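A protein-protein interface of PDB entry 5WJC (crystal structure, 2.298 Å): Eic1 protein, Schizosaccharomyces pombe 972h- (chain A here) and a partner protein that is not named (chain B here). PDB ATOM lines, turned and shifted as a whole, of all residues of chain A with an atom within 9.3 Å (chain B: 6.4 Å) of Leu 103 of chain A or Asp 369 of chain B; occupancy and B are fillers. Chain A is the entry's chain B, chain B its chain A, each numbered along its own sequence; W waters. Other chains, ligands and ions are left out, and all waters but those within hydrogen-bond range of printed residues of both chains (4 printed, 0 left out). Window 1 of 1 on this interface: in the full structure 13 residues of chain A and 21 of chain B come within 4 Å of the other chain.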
ATOM      1  N   ASN A  99       1.100 -13.999 -10.568  1.00  0.00           N
ATOM      2  CA  ASN A  99       0.015 -13.023 -10.634  1.00  0.00           C
ATOM      3  C   ASN A  99       0.073 -12.186 -11.908  1.00  0.00           C
ATOM      4  O   ASN A  99       0.823 -11.213 -11.982  1.00  0.00           O
ATOM      5  CB  ASN A  99       0.057 -12.098  -9.414  1.00  0.00           C
ATOM      6  CG  ASN A  99       0.217 -12.859  -8.117  1.00  0.00           C
ATOM      7  OD1 ASN A  99      -0.584 -13.749  -7.806  1.00  0.00           O
ATOM      8  ND2 ASN A  99       1.253 -12.515  -7.346  1.00  0.00           N
ATOM      9  N   ARG A 100      -0.732 -12.557 -12.897  1.00  0.00           N
ATOM     10  CA  ARG A 100      -0.752 -11.831 -14.157  1.00  0.00           C
ATOM     11  C   ARG A 100      -0.974 -10.347 -13.915  1.00  0.00           C
ATOM     12  O   ARG A 100      -1.783  -9.953 -13.065  1.00  0.00           O
ATOM     13  CB  ARG A 100      -1.852 -12.381 -15.067  1.00  0.00           C
ATOM     14  CG  ARG A 100      -2.230 -13.807 -14.757  1.00  0.00           C
ATOM     15  CD  ARG A 100      -3.029 -14.411 -15.888  1.00  0.00           C
ATOM     16  NE  ARG A 100      -2.222 -14.554 -17.109  1.00  0.00           N
ATOM     17  CZ  ARG A 100      -1.244 -15.443 -17.296  1.00  0.00           C
ATOM     18  NH1 ARG A 100      -0.598 -15.469 -18.461  1.00  0.00           N
ATOM     19  NH2 ARG A 100      -0.909 -16.308 -16.338  1.00  0.00           N
ATOM     20  N   VAL A 101      -0.204  -9.528 -14.633  1.00  0.00           N
ATOM     21  CA  VAL A 101      -0.482  -8.103 -14.715  1.00  0.00           C
ATOM     22  C   VAL A 101      -1.151  -7.748 -16.039  1.00  0.00           C
ATOM     23  O   VAL A 101      -1.724  -6.651 -16.160  1.00  0.00           O
ATOM     24  CB  VAL A 101       0.798  -7.265 -14.470  1.00  0.00           C
ATOM     25  CG1 VAL A 101       1.699  -7.260 -15.673  1.00  0.00           C
ATOM     26  CG2 VAL A 101       0.442  -5.838 -14.074  1.00  0.00           C
ATOM     27  N   PHE A 102      -1.129  -8.655 -17.013  1.00  0.00           N
ATOM     28  CA  PHE A 102      -1.893  -8.541 -18.249  1.00  0.00           C
ATOM     29  C   PHE A 102      -2.057  -9.944 -18.820  1.00  0.00           C
ATOM     30  O   PHE A 102      -1.375 -10.888 -18.410  1.00  0.00           O
ATOM     31  CB  PHE A 102      -1.212  -7.610 -19.258  1.00  0.00           C
ATOM     32  CG  PHE A 102       0.200  -8.027 -19.618  1.00  0.00           C
ATOM     33  CD1 PHE A 102       0.437  -8.949 -20.631  1.00  0.00           C
ATOM     34  CD2 PHE A 102       1.287  -7.491 -18.948  1.00  0.00           C
ATOM     35  CE1 PHE A 102       1.742  -9.329 -20.962  1.00  0.00           C
ATOM     36  CE2 PHE A 102       2.585  -7.873 -19.268  1.00  0.00           C
ATOM     37  CZ  PHE A 102       2.811  -8.794 -20.276  1.00  0.00           C
ATOM     38  N   LEU A 103      -2.983 -10.077 -19.764  1.00  0.00           N
ATOM     39  CA  LEU A 103      -3.221 -11.357 -20.421  1.00  0.00           C
ATOM     40  C   LEU A 103      -2.284 -11.486 -21.618  1.00  0.00           C
ATOM     41  O   LEU A 103      -2.250 -10.605 -22.488  1.00  0.00           O
ATOM     42  CB  LEU A 103      -4.679 -11.489 -20.863  1.00  0.00           C
ATOM     43  CG  LEU A 103      -5.778 -11.138 -19.840  1.00  0.00           C
ATOM     44  CD1 LEU A 103      -7.147 -11.579 -20.360  1.00  0.00           C
ATOM     45  CD2 LEU A 103      -5.519 -11.712 -18.440  1.00  0.00           C
ATOM     46  N   ARG A 104      -1.509 -12.572 -21.648  1.00  0.00           N
ATOM     47  CA  ARG A 104      -0.586 -12.782 -22.757  1.00  0.00           C
ATOM     48  C   ARG A 104      -1.323 -12.983 -24.077  1.00  0.00           C
ATOM     49  O   ARG A 104      -0.849 -12.526 -25.123  1.00  0.00           O
ATOM     50  CB  ARG A 104       0.334 -13.967 -22.459  1.00  0.00           C
ATOM     51  CG  ARG A 104       1.368 -13.650 -21.392  1.00  0.00           C
ATOM     52  CD  ARG A 104       2.357 -14.790 -21.229  1.00  0.00           C
ATOM     53  NE  ARG A 104       1.703 -15.971 -20.665  1.00  0.00           N
ATOM     54  CZ  ARG A 104       2.216 -16.739 -19.705  1.00  0.00           C
ATOM     55  NH1 ARG A 104       3.410 -16.462 -19.183  1.00  0.00           N
ATOM     56  NH2 ARG A 104       1.529 -17.791 -19.267  1.00  0.00           N
ATOM     57  N   ARG A 105      -2.492 -13.623 -24.055  1.00  0.00           N
ATOM     58  CA  ARG A 105      -3.245 -13.770 -25.294  1.00  0.00           C
ATOM     59  C   ARG A 105      -3.683 -12.417 -25.859  1.00  0.00           C
ATOM     60  O   ARG A 105      -3.845 -12.293 -27.080  1.00  0.00           O
ATOM     61  CB  ARG A 105      -4.442 -14.690 -25.077  1.00  0.00           C
ATOM     62  CG  ARG A 105      -5.469 -14.188 -24.078  1.00  0.00           C
ATOM     63  CD  ARG A 105      -6.338 -15.337 -23.561  1.00  0.00           C
ATOM     64  NE  ARG A 105      -7.423 -14.838 -22.721  1.00  0.00           N
ATOM     65  CZ  ARG A 105      -8.037 -15.545 -21.779  1.00  0.00           C
ATOM     66  NH1 ARG A 105      -7.674 -16.797 -21.538  1.00  0.00           N
ATOM     67  NH2 ARG A 105      -9.016 -14.994 -21.069  1.00  0.00           N
ATOM     68  N   ASN A 106      -3.863 -11.396 -25.004  1.00  0.00           N
ATOM     69  CA  ASN A 106      -4.113 -10.043 -25.503  1.00  0.00           C
ATOM     70  C   ASN A 106      -2.926  -9.536 -26.319  1.00  0.00           C
ATOM     71  O   ASN A 106      -3.101  -9.010 -27.429  1.00  0.00           O
ATOM     72  CB  ASN A 106      -4.378  -9.066 -24.353  1.00  0.00           C
ATOM     73  CG  ASN A 106      -5.733  -9.252 -23.683  1.00  0.00           C
ATOM     74  OD1 ASN A 106      -5.963  -8.671 -22.616  1.00  0.00           O
ATOM     75  ND2 ASN A 106      -6.624 -10.044 -24.284  1.00  0.00           N
ATOM     76  N   VAL A 107      -1.708  -9.646 -25.762  1.00  0.00           N
ATOM     77  CA  VAL A 107      -0.510  -9.206 -26.484  1.00  0.00           C
ATOM     78  C   VAL A 107      -0.362  -9.982 -27.791  1.00  0.00           C
ATOM     79  O   VAL A 107      -0.143  -9.394 -28.855  1.00  0.00           O
ATOM     80  CB  VAL A 107       0.746  -9.341 -25.605  1.00  0.00           C
ATOM     81  CG1 VAL A 107       2.002  -9.000 -26.419  1.00  0.00           C
ATOM     82  CG2 VAL A 107       0.645  -8.430 -24.395  1.00  0.00           C
ATOM     83  N   ARG A 108      -0.508 -11.310 -27.732  1.00  0.00           N
ATOM     84  CA  ARG A 108      -0.429 -12.118 -28.947  1.00  0.00           C
ATOM     85  C   ARG A 108      -1.413 -11.632 -30.007  1.00  0.00           C
ATOM     86  O   ARG A 108      -1.074 -11.571 -31.196  1.00  0.00           O
ATOM     87  CB  ARG A 108      -0.676 -13.591 -28.619  1.00  0.00           C
ATOM     88  CG  ARG A 108       0.572 -14.317 -28.111  1.00  0.00           C
ATOM     89  CD  ARG A 108       0.445 -15.832 -28.187  1.00  0.00           C
ATOM     90  NE  ARG A 108      -0.624 -16.335 -27.330  1.00  0.00           N
ATOM     91  CZ  ARG A 108      -0.532 -16.451 -26.006  1.00  0.00           C
ATOM     92  NH1 ARG A 108       0.589 -16.096 -25.376  1.00  0.00           N
ATOM     93  NH2 ARG A 108      -1.565 -16.923 -25.309  1.00  0.00           N
ATOM     94  N   ALA A 109      -2.632 -11.268 -29.596  1.00  0.00           N
ATOM     95  CA  ALA A 109      -3.624 -10.767 -30.548  1.00  0.00           C
ATOM     96  C   ALA A 109      -3.200  -9.435 -31.159  1.00  0.00           C
ATOM     97  O   ALA A 109      -3.419  -9.193 -32.351  1.00  0.00           O
ATOM     98  CB  ALA A 109      -4.979 -10.620 -29.861  1.00  0.00           C
ATOM     99  N   VAL A 110      -2.589  -8.558 -30.360  1.00  0.00           N
ATOM    100  CA  VAL A 110      -2.278  -7.216 -30.840  1.00  0.00           C
ATOM    101  C   VAL A 110      -0.967  -7.202 -31.620  1.00  0.00           C
ATOM    102  O   VAL A 110      -0.833  -6.473 -32.612  1.00  0.00           O
ATOM    103  CB  VAL A 110      -2.252  -6.224 -29.661  1.00  0.00           C
ATOM    104  CG1 VAL A 110      -1.910  -4.837 -30.142  1.00  0.00           C
ATOM    105  CG2 VAL A 110      -3.592  -6.206 -28.938  1.00  0.00           C
ATOM    106  N   LEU B  40      -1.270  -3.346 -25.767  1.00  0.00           N
ATOM    107  CA  LEU B  40      -2.446  -3.635 -24.952  1.00  0.00           C
ATOM    108  C   LEU B  40      -3.510  -2.557 -25.095  1.00  0.00           C
ATOM    109  O   LEU B  40      -4.706  -2.863 -25.082  1.00  0.00           O
ATOM    110  CB  LEU B  40      -2.052  -3.783 -23.480  1.00  0.00           C
ATOM    111  CG  LEU B  40      -1.312  -5.070 -23.113  1.00  0.00           C
ATOM    112  CD1 LEU B  40      -0.745  -4.980 -21.691  1.00  0.00           C
ATOM    113  CD2 LEU B  40      -2.242  -6.269 -23.270  1.00  0.00           C
ATOM    114  N   GLN B 362     -10.840 -23.215 -25.765  1.00  0.00           N
ATOM    115  CA  GLN B 362      -9.540 -22.586 -25.609  1.00  0.00           C
ATOM    116  C   GLN B 362      -8.429 -23.556 -25.981  1.00  0.00           C
ATOM    117  O   GLN B 362      -8.582 -24.779 -25.875  1.00  0.00           O
ATOM    118  CB  GLN B 362      -9.295 -22.129 -24.171  1.00  0.00           C
ATOM    119  CG  GLN B 362     -10.225 -21.070 -23.649  1.00  0.00           C
ATOM    120  CD  GLN B 362      -9.960 -20.783 -22.189  1.00  0.00           C
ATOM    121  OE1 GLN B 362     -10.164 -21.648 -21.326  1.00  0.00           O
ATOM    122  NE2 GLN B 362      -9.500 -19.571 -21.897  1.00  0.00           N
ATOM    123  N   PRO B 364      -4.537 -24.766 -24.862  1.00  0.00           N
ATOM    124  CA  PRO B 364      -3.790 -24.759 -23.593  1.00  0.00           C
ATOM    125  C   PRO B 364      -3.032 -23.471 -23.350  1.00  0.00           C
ATOM    126  O   PRO B 364      -3.037 -22.962 -22.222  1.00  0.00           O
ATOM    127  CB  PRO B 364      -2.847 -25.961 -23.745  1.00  0.00           C
ATOM    128  CG  PRO B 364      -3.587 -26.881 -24.669  1.00  0.00           C
ATOM    129  CD  PRO B 364      -4.283 -25.986 -25.651  1.00  0.00           C
ATOM    130  N   GLU B 365      -2.382 -22.922 -24.378  1.00  0.00           N
ATOM    131  CA  GLU B 365      -1.611 -21.703 -24.170  1.00  0.00           C
ATOM    132  C   GLU B 365      -2.525 -20.513 -23.881  1.00  0.00           C
ATOM    133  O   GLU B 365      -2.188 -19.663 -23.050  1.00  0.00           O
ATOM    134  CB  GLU B 365      -0.691 -21.447 -25.376  1.00  0.00           C
ATOM    135  CG  GLU B 365      -1.171 -20.385 -26.372  1.00  0.00           C
ATOM    136  CD  GLU B 365      -0.074 -19.868 -27.318  1.00  0.00           C
ATOM    137  OE1 GLU B 365      -0.385 -19.650 -28.515  1.00  0.00           O
ATOM    138  OE2 GLU B 365       1.083 -19.672 -26.869  1.00  0.00           O
ATOM    139  N   ASP B 366      -3.696 -20.450 -24.519  1.00  0.00           N
ATOM    140  CA  ASP B 366      -4.637 -19.382 -24.194  1.00  0.00           C
ATOM    141  C   ASP B 366      -5.214 -19.569 -22.795  1.00  0.00           C
ATOM    142  O   ASP B 366      -5.345 -18.600 -22.043  1.00  0.00           O
ATOM    143  CB  ASP B 366      -5.750 -19.325 -25.240  1.00  0.00           C
ATOM    144  CG  ASP B 366      -5.331 -18.558 -26.499  1.00  0.00           C
ATOM    145  OD1 ASP B 366      -4.197 -18.010 -26.520  1.00  0.00           O
ATOM    146  OD2 ASP B 366      -6.129 -18.511 -27.470  1.00  0.00           O
ATOM    147  N   ALA B 367      -5.521 -20.815 -22.415  1.00  0.00           N
ATOM    148  CA  ALA B 367      -6.064 -21.120 -21.092  1.00  0.00           C
ATOM    149  C   ALA B 367      -5.139 -20.700 -19.956  1.00  0.00           C
ATOM    150  O   ALA B 367      -5.608 -20.542 -18.825  1.00  0.00           O
ATOM    151  CB  ALA B 367      -6.366 -22.614 -20.980  1.00  0.00           C
ATOM    152  N   GLU B 368      -3.841 -20.511 -20.220  1.00  0.00           N
ATOM    153  CA  GLU B 368      -2.935 -20.040 -19.175  1.00  0.00           C
ATOM    154  C   GLU B 368      -3.312 -18.664 -18.639  1.00  0.00           C
ATOM    155  O   GLU B 368      -2.855 -18.294 -17.553  1.00  0.00           O
ATOM    156  CB  GLU B 368      -1.490 -20.004 -19.688  1.00  0.00           C
ATOM    157  CG  GLU B 368      -1.069 -21.246 -20.475  1.00  0.00           C
ATOM    158  CD  GLU B 368       0.432 -21.302 -20.780  1.00  0.00           C
ATOM    159  OE1 GLU B 368       0.912 -22.376 -21.230  1.00  0.00           O
ATOM    160  OE2 GLU B 368       1.128 -20.281 -20.568  1.00  0.00           O
ATOM    161  N   ASP B 369      -4.117 -17.889 -19.369  1.00  0.00           N
ATOM    162  CA  ASP B 369      -4.515 -16.563 -18.911  1.00  0.00           C
ATOM    163  C   ASP B 369      -5.800 -16.570 -18.091  1.00  0.00           C
ATOM    164  O   ASP B 369      -6.146 -15.534 -17.510  1.00  0.00           O
ATOM    165  CB  ASP B 369      -4.691 -15.603 -20.100  1.00  0.00           C
ATOM    166  CG  ASP B 369      -3.370 -15.218 -20.754  1.00  0.00           C
ATOM    167  OD1 ASP B 369      -3.276 -15.329 -22.005  1.00  0.00           O
ATOM    168  OD2 ASP B 369      -2.429 -14.796 -20.031  1.00  0.00           O
ATOM    169  N   GLY B 370      -6.508 -17.693 -18.026  1.00  0.00           N
ATOM    170  CA  GLY B 370      -7.768 -17.796 -17.319  1.00  0.00           C
ATOM    171  C   GLY B 370      -8.910 -18.119 -18.260  1.00  0.00           C
ATOM    172  O   GLY B 370      -8.721 -18.421 -19.442  1.00  0.00           O
ATOM    173  N   SER B 371     -10.125 -18.050 -17.711  1.00  0.00           N
ATOM    174  CA  SER B 371     -11.318 -18.406 -18.452  1.00  0.00           C
ATOM    175  C   SER B 371     -11.480 -17.503 -19.676  1.00  0.00           C
ATOM    176  O   SER B 371     -10.956 -16.387 -19.711  1.00  0.00           O
ATOM    177  CB  SER B 371     -12.542 -18.307 -17.547  1.00  0.00           C
ATOM    178  OG  SER B 371     -12.606 -17.026 -16.951  1.00  0.00           O
ATOM    179  N   LEU B 374     -12.869 -13.781 -19.616  1.00  0.00           N
ATOM    180  CA  LEU B 374     -12.032 -12.680 -19.134  1.00  0.00           C
ATOM    181  C   LEU B 374     -11.406 -12.006 -20.352  1.00  0.00           C
ATOM    182  O   LEU B 374     -10.455 -12.516 -20.944  1.00  0.00           O
ATOM    183  CB  LEU B 374     -10.981 -13.190 -18.154  1.00  0.00           C
ATOM    184  CG  LEU B 374      -9.986 -12.174 -17.599  1.00  0.00           C
ATOM    185  CD1 LEU B 374     -10.735 -11.050 -16.928  1.00  0.00           C
ATOM    186  CD2 LEU B 374      -9.052 -12.854 -16.619  1.00  0.00           C
ATOM    187  N   LEU B 375     -11.953 -10.861 -20.752  1.00  0.00           N
ATOM    188  CA  LEU B 375     -11.517 -10.267 -22.009  1.00  0.00           C
ATOM    189  C   LEU B 375     -10.194  -9.526 -21.859  1.00  0.00           C
ATOM    190  O   LEU B 375      -9.308  -9.634 -22.718  1.00  0.00           O
ATOM    191  CB  LEU B 375     -12.595  -9.320 -22.532  1.00  0.00           C
ATOM    192  CG  LEU B 375     -12.307  -8.633 -23.865  1.00  0.00           C
ATOM    193  CD1 LEU B 375     -12.110  -9.658 -24.985  1.00  0.00           C
ATOM    194  CD2 LEU B 375     -13.443  -7.669 -24.181  1.00  0.00           C
ATOM    195  N   PHE B 376     -10.032  -8.782 -20.776  1.00  0.00           N
ATOM    196  CA  PHE B 376      -8.917  -7.856 -20.696  1.00  0.00           C
ATOM    197  C   PHE B 376      -8.634  -7.582 -19.231  1.00  0.00           C
ATOM    198  O   PHE B 376      -9.562  -7.535 -18.416  1.00  0.00           O
ATOM    199  CB  PHE B 376      -9.252  -6.558 -21.442  1.00  0.00           C
ATOM    200  CG  PHE B 376      -8.143  -5.552 -21.449  1.00  0.00           C
ATOM    201  CD1 PHE B 376      -7.148  -5.613 -22.397  1.00  0.00           C
ATOM    202  CD2 PHE B 376      -8.111  -4.529 -20.511  1.00  0.00           C
ATOM    203  CE1 PHE B 376      -6.123  -4.681 -22.407  1.00  0.00           C
ATOM    204  CE2 PHE B 376      -7.096  -3.588 -20.513  1.00  0.00           C
ATOM    205  CZ  PHE B 376      -6.098  -3.658 -21.458  1.00  0.00           C
ATOM    206  N   MET B 377      -7.357  -7.424 -18.901  1.00  0.00           N
ATOM    207  CA  MET B 377      -6.931  -7.084 -17.547  1.00  0.00           C
ATOM    208  C   MET B 377      -6.126  -5.793 -17.591  1.00  0.00           C
ATOM    209  O   MET B 377      -5.138  -5.703 -18.324  1.00  0.00           O
ATOM    210  CB  MET B 377      -6.095  -8.207 -16.932  1.00  0.00           C
ATOM    211  CG  MET B 377      -5.509  -7.851 -15.566  1.00  0.00           C
ATOM    212  SD  MET B 377      -4.411  -9.129 -14.883  1.00  0.00           S
ATOM    213  CE  MET B 377      -5.599 -10.314 -14.245  1.00  0.00           C
HETATM  214  O   HOH W   1      -9.213 -18.033 -24.211  1.00  0.00           O
HETATM  215  O   HOH W   2      -2.735  -4.736 -18.165  1.00  0.00           O
HETATM  216  O   HOH W   3      -9.016 -12.343 -23.965  1.00  0.00           O
HETATM  217  O   HOH W   4      -4.605  -7.940 -20.413  1.00  0.00           O
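Water W2 lies within hydrogen-bond range of the backbone carbonyl oxygen (O) of Met 377 of chain B (2.6 Å) and the backbone carbonyl oxygen (O) of Val 101 of chain A (3.0 Å). Water W4 lies within hydrogen-bond range of the side-chain amide oxygen (OD1) of Asn 106 of chain A (2.7 Å), the backbone NH (N) of Leu 103 of chain A (2.8 Å) and the backbone carbonyl oxygen (O) of Met 377 of chain B (3.1 Å). Water W1 bridges NE2 of Gln 362 of chain B (2.8 Å) and NH1 of Arg 105 of chain A (3.3 Å). Water W3 lies within hydrogen-bond range of the backbone carbonyl oxygen (O) of Leu 375 of chain B (3.0 Å), the guanidinium group (NE) of Arg 105 of chain A (3.2 Å), the side-chain amide nitrogen (ND2) of Asn 106 of chain A (3.3 Å) and the backbone carbonyl oxygen (O) of Leu 374 of chain B (3.4 Å).
The backbone carbonyl oxygen (O) of Gly 370 of chain B sits at hydrogen-bond distance from the side-chain amide nitrogen (NE2) of Gln 362 of chain B (2.8 Å).
Hydrophobic or aromatic side chains of chain A within 4 Å of the printed part of chain B: Phe 102, Leu 103 and Val 107. Hydrophobic or aromatic side chains of chain B that line the printed part of chain A: Leu 40, Leu 374, Phe 376 and Met 377.
Among the printed residues, merely in contact across the chains: Val 101 of chain A with Met 377 of chain B, Phe 102 of chain A with Leu 40 of chain B, Phe 102 of chain A with Met 377 of chain B, Leu 103 of chain A with Asp 369 of chain B, Leu 103 of chain A with Leu 374 of chain B, Leu 103 of chain A with Leu 375 of chain B, Leu 103 of chain A with Met 377 of chain B, Asn 106 of chain A with Leu 40 of chain B, Asn 106 of chain A with Phe 376 of chain B and Val 107 of chain A with Leu 40 of chain B.
The backbone carbonyl oxygen of Arg 100 of chain A sits close to the side-chain sulfur of Met 377 of chain B, 3.3 Å away. N of Arg 104 of chain A lies within hydrogen-bond range of OD2 of Asp 369 of chain B, 2.9 Å away. The backbone carbonyl oxygen (O) of Ser 371 of chain B is in hydrogen-bond range of the guanidinium group (NH2) of Arg 105 of chain A (2.7 Å). The backbone carbonyl oxygen (O) of Gly 370 of chain B sits at hydrogen-bond distance from the guanidinium group (NH1) of Arg 105 of chain A (2.9 Å). The backbone carbonyl oxygen of Leu 375 of chain B lies within hydrogen-bond range of the side-chain amide nitrogen of Asn 106 of chain A, 3.1 Å away. OE1 of Glu 365 of chain B is in salt-bridge range of NE of Arg 108 of chain A (3.5 Å). N of Arg 105 of chain A is in hydrogen-bond range of OD1 of Asp 369 of chain B (2.8 Å). The guanidinium group of Arg 108 of chain A lies within salt-bridge range of the side-chain carboxylate of Asp 366 of chain B, at 3.1 Å. The guanidinium group of Arg 100 of chain A is in hydrogen-bond range of the backbone carbonyl oxygen of Glu 368 of chain B, 3.0 Å away. The backbone carbonyl oxygen of Asp 366 of chain B is in hydrogen-bond range of the guanidinium group of Arg 105 of chain A, at 3.0 Å. The guanidinium group of Arg 104 of chain A is in salt-bridge range of the side-chain carboxylate of Glu 368 of chain B, at 2.8 Å. The backbone carbonyl oxygen of Leu 374 of chain B lies within hydrogen-bond range of the guanidinium group of Arg 105 of chain A (2.9 Å). The side-chain amide nitrogen (NE2) of Gln 362 of chain B sits close to the guanidinium group (NH1) of Arg 105 of chain A (3.3 Å). NH1 of Arg 100 of chain A is in salt-bridge range of OD2 of Asp 369 of chain B (2.5 Å).
Asn 99 of chain A touches none of the printed residues of chain B. Of the printed residues of chain B, Leu 103 of chain A touches Asp 369 (3.6 Å), Leu 374 (3.5 Å), Leu 375 (3.7 Å) and Met 377 (3.9 Å). Printed residues of chain B within 4 Å of Arg 108 of chain A: Glu 365 and Asp 366. Ala 109 of chain A touches none of the printed residues of chain B. Printed residues of chain A within 4 Å of Leu 40 of chain B: Phe 102 (3.6 Å), Asn 106 (3.7 Å) and Val 107 (3.8 Å). Printed residues of chain A within 4 Å of Asp 366 of chain B: Arg 105 and Arg 108. Asp 369 of chain B touches four residues of chain A. Gly 370 of chain B touches one residue of chain A. Of the printed residues of chain A, Met 377 of chain B touches Arg 100, Val 101, Phe 102 and Leu 103.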
